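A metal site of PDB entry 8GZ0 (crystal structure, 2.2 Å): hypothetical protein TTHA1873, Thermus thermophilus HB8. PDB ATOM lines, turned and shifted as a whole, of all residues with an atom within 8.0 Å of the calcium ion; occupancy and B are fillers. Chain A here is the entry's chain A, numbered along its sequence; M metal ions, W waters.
N of Asp 95 lies within hydrogen-bond range of O of Thr 136 (2.9 Å).
Of the 15 residues printed, 5 come within 4 Å of the calcium ion.
OD1 of Asp 97 is bound to the calcium ion.
The calcium ion is bound by water W1 (2.3 Å).
The calcium ion is bound by O of Gly 98, 2.3 Å away.
The calcium ion is bound by the backbone carbonyl oxygen (O) of Ala 103, 2.3 Å away.
The calcium ion is bound by the backbone carbonyl oxygen (O) of Gly 101, 2.4 Å away.
The calcium ion is bound by the side-chain carboxylate (OD1) of Asp 95, 2.4 Å away.
OD2 of Asp 95 is bound to the calcium ion (2.6 Å).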
ATOM      1  N   LEU A  94      11.502  29.274   3.308  1.00  0.00           N
ATOM      2  CA  LEU A  94      12.080  28.081   2.704  1.00  0.00           C
ATOM      3  C   LEU A  94      12.304  28.321   1.199  1.00  0.00           C
ATOM      4  O   LEU A  94      11.389  28.740   0.490  1.00  0.00           O
ATOM      5  CB  LEU A  94      11.153  26.866   2.907  1.00  0.00           C
ATOM      6  CG  LEU A  94      11.568  25.580   2.171  1.00  0.00           C
ATOM      7  CD1 LEU A  94      12.829  24.988   2.777  1.00  0.00           C
ATOM      8  CD2 LEU A  94      10.444  24.531   2.170  1.00  0.00           C
ATOM      9  N   ASP A  95      13.534  28.033   0.751  1.00  0.00           N
ATOM     10  CA  ASP A  95      13.849  27.899  -0.663  1.00  0.00           C
ATOM     11  C   ASP A  95      14.038  26.407  -0.910  1.00  0.00           C
ATOM     12  O   ASP A  95      15.099  25.863  -0.594  1.00  0.00           O
ATOM     13  CB  ASP A  95      15.100  28.698  -1.064  1.00  0.00           C
ATOM     14  CG  ASP A  95      15.434  28.559  -2.546  1.00  0.00           C
ATOM     15  OD1 ASP A  95      14.856  27.684  -3.205  1.00  0.00           O
ATOM     16  OD2 ASP A  95      16.274  29.324  -3.043  1.00  0.00           O
ATOM     17  N   PRO A  96      13.033  25.711  -1.484  1.00  0.00           N
ATOM     18  CA  PRO A  96      12.973  24.258  -1.393  1.00  0.00           C
ATOM     19  C   PRO A  96      14.101  23.547  -2.136  1.00  0.00           C
ATOM     20  O   PRO A  96      14.388  22.407  -1.781  1.00  0.00           O
ATOM     21  CB  PRO A  96      11.573  23.923  -1.960  1.00  0.00           C
ATOM     22  CG  PRO A  96      11.251  25.096  -2.861  1.00  0.00           C
ATOM     23  CD  PRO A  96      11.899  26.298  -2.208  1.00  0.00           C
ATOM     24  N   ASP A  97      14.735  24.223  -3.122  1.00  0.00           N
ATOM     25  CA  ASP A  97      15.815  23.658  -3.923  1.00  0.00           C
ATOM     26  C   ASP A  97      17.113  24.445  -3.726  1.00  0.00           C
ATOM     27  O   ASP A  97      18.083  24.245  -4.439  1.00  0.00           O
ATOM     28  CB  ASP A  97      15.422  23.591  -5.387  1.00  0.00           C
ATOM     29  CG  ASP A  97      14.959  24.895  -6.044  1.00  0.00           C
ATOM     30  OD1 ASP A  97      15.195  25.979  -5.451  1.00  0.00           O
ATOM     31  OD2 ASP A  97      14.395  24.818  -7.165  1.00  0.00           O
ATOM     32  N   GLY A  98      17.117  25.377  -2.762  1.00  0.00           N
ATOM     33  CA  GLY A  98      18.300  26.162  -2.456  1.00  0.00           C
ATOM     34  C   GLY A  98      18.837  26.910  -3.670  1.00  0.00           C
ATOM     35  O   GLY A  98      18.098  27.354  -4.531  1.00  0.00           O
ATOM     36  N   PRO A  99      20.180  27.066  -3.782  1.00  0.00           N
ATOM     37  CA  PRO A  99      20.782  27.652  -4.978  1.00  0.00           C
ATOM     38  C   PRO A  99      20.807  26.723  -6.200  1.00  0.00           C
ATOM     39  O   PRO A  99      21.298  27.134  -7.255  1.00  0.00           O
ATOM     40  CB  PRO A  99      22.221  27.936  -4.499  1.00  0.00           C
ATOM     41  CG  PRO A  99      22.515  26.845  -3.467  1.00  0.00           C
ATOM     42  CD  PRO A  99      21.184  26.652  -2.781  1.00  0.00           C
ATOM     43  N   PHE A 100      20.318  25.481  -6.043  1.00  0.00           N
ATOM     44  CA  PHE A 100      20.480  24.436  -7.056  1.00  0.00           C
ATOM     45  C   PHE A 100      19.364  24.498  -8.087  1.00  0.00           C
ATOM     46  O   PHE A 100      19.481  23.904  -9.162  1.00  0.00           O
ATOM     47  CB  PHE A 100      20.544  23.065  -6.374  1.00  0.00           C
ATOM     48  CG  PHE A 100      21.705  22.962  -5.410  1.00  0.00           C
ATOM     49  CD1 PHE A 100      23.002  22.838  -5.884  1.00  0.00           C
ATOM     50  CD2 PHE A 100      21.491  23.074  -4.048  1.00  0.00           C
ATOM     51  CE1 PHE A 100      24.080  22.795  -4.997  1.00  0.00           C
ATOM     52  CE2 PHE A 100      22.567  23.051  -3.170  1.00  0.00           C
ATOM     53  CZ  PHE A 100      23.857  22.905  -3.636  1.00  0.00           C
ATOM     54  N   GLY A 101      18.299  25.233  -7.749  1.00  0.00           N
ATOM     55  CA  GLY A 101      17.142  25.363  -8.609  1.00  0.00           C
ATOM     56  C   GLY A 101      16.485  26.740  -8.468  1.00  0.00           C
ATOM     57  O   GLY A 101      16.696  27.453  -7.493  1.00  0.00           O
ATOM     58  N   PRO A 102      15.657  27.133  -9.461  1.00  0.00           N
ATOM     59  CA  PRO A 102      15.067  28.465  -9.486  1.00  0.00           C
ATOM     60  C   PRO A 102      13.791  28.703  -8.652  1.00  0.00           C
ATOM     61  O   PRO A 102      13.217  29.776  -8.719  1.00  0.00           O
ATOM     62  CB  PRO A 102      14.739  28.633 -10.972  1.00  0.00           C
ATOM     63  CG  PRO A 102      14.449  27.242 -11.456  1.00  0.00           C
ATOM     64  CD  PRO A 102      15.270  26.305 -10.612  1.00  0.00           C
ATOM     65  N   ALA A 103      13.380  27.725  -7.849  1.00  0.00           N
ATOM     66  CA  ALA A 103      12.357  27.999  -6.866  1.00  0.00           C
ATOM     67  C   ALA A 103      12.853  29.147  -5.970  1.00  0.00           C
ATOM     68  O   ALA A 103      14.041  29.213  -5.660  1.00  0.00           O
ATOM     69  CB  ALA A 103      12.038  26.763  -6.066  1.00  0.00           C
ATOM     70  N   SER A 104      11.919  30.044  -5.580  1.00  0.00           N
ATOM     71  CA  SER A 104      12.218  31.191  -4.735  1.00  0.00           C
ATOM     72  C   SER A 104      11.958  30.876  -3.258  1.00  0.00           C
ATOM     73  O   SER A 104      11.250  29.926  -2.938  1.00  0.00           O
ATOM     74  CB  SER A 104      11.365  32.352  -5.169  1.00  0.00           C
ATOM     75  OG  SER A 104      11.879  32.903  -6.345  1.00  0.00           O
ATOM     76  N   TYR A 105      12.471  31.743  -2.375  1.00  0.00           N
ATOM     77  CA  TYR A 105      12.059  31.801  -0.986  1.00  0.00           C
ATOM     78  C   TYR A 105      10.561  32.157  -0.864  1.00  0.00           C
ATOM     79  O   TYR A 105      10.063  33.031  -1.587  1.00  0.00           O
ATOM     80  CB  TYR A 105      12.919  32.811  -0.219  1.00  0.00           C
ATOM     81  CG  TYR A 105      14.226  32.289   0.335  1.00  0.00           C
ATOM     82  CD1 TYR A 105      14.226  31.333   1.334  1.00  0.00           C
ATOM     83  CD2 TYR A 105      15.451  32.732  -0.137  1.00  0.00           C
ATOM     84  CE1 TYR A 105      15.407  30.853   1.857  1.00  0.00           C
ATOM     85  CE2 TYR A 105      16.647  32.245   0.357  1.00  0.00           C
ATOM     86  CZ  TYR A 105      16.632  31.306   1.375  1.00  0.00           C
ATOM     87  OH  TYR A 105      17.794  30.812   1.905  1.00  0.00           O
ATOM     88  N   GLY A 134      20.060  20.172   0.124  1.00  0.00           N
ATOM     89  CA  GLY A 134      20.163  21.276  -0.836  1.00  0.00           C
ATOM     90  C   GLY A 134      19.259  22.463  -0.499  1.00  0.00           C
ATOM     91  O   GLY A 134      19.601  23.606  -0.827  1.00  0.00           O
ATOM     92  N   ALA A 135      18.133  22.203   0.185  1.00  0.00           N
ATOM     93  CA  ALA A 135      17.205  23.253   0.573  1.00  0.00           C
ATOM     94  C   ALA A 135      17.828  24.214   1.604  1.00  0.00           C
ATOM     95  O   ALA A 135      18.699  23.826   2.391  1.00  0.00           O
ATOM     96  CB  ALA A 135      15.928  22.648   1.102  1.00  0.00           C
ATOM     97  N   THR A 136      17.352  25.475   1.577  1.00  0.00           N
ATOM     98  CA  THR A 136      17.824  26.507   2.495  1.00  0.00           C
ATOM     99  C   THR A 136      16.644  27.190   3.201  1.00  0.00           C
ATOM    100  O   THR A 136      15.535  27.297   2.666  1.00  0.00           O
ATOM    101  CB  THR A 136      18.737  27.523   1.797  1.00  0.00           C
ATOM    102  OG1 THR A 136      17.935  28.351   0.949  1.00  0.00           O
ATOM    103  CG2 THR A 136      19.877  26.866   1.049  1.00  0.00           C
HETATM  104 CA    CA M   1      16.018  28.007  -5.281  1.00  0.00          CA
HETATM  105  O   HOH W   1      17.186  29.750  -6.116  1.00  0.00           O
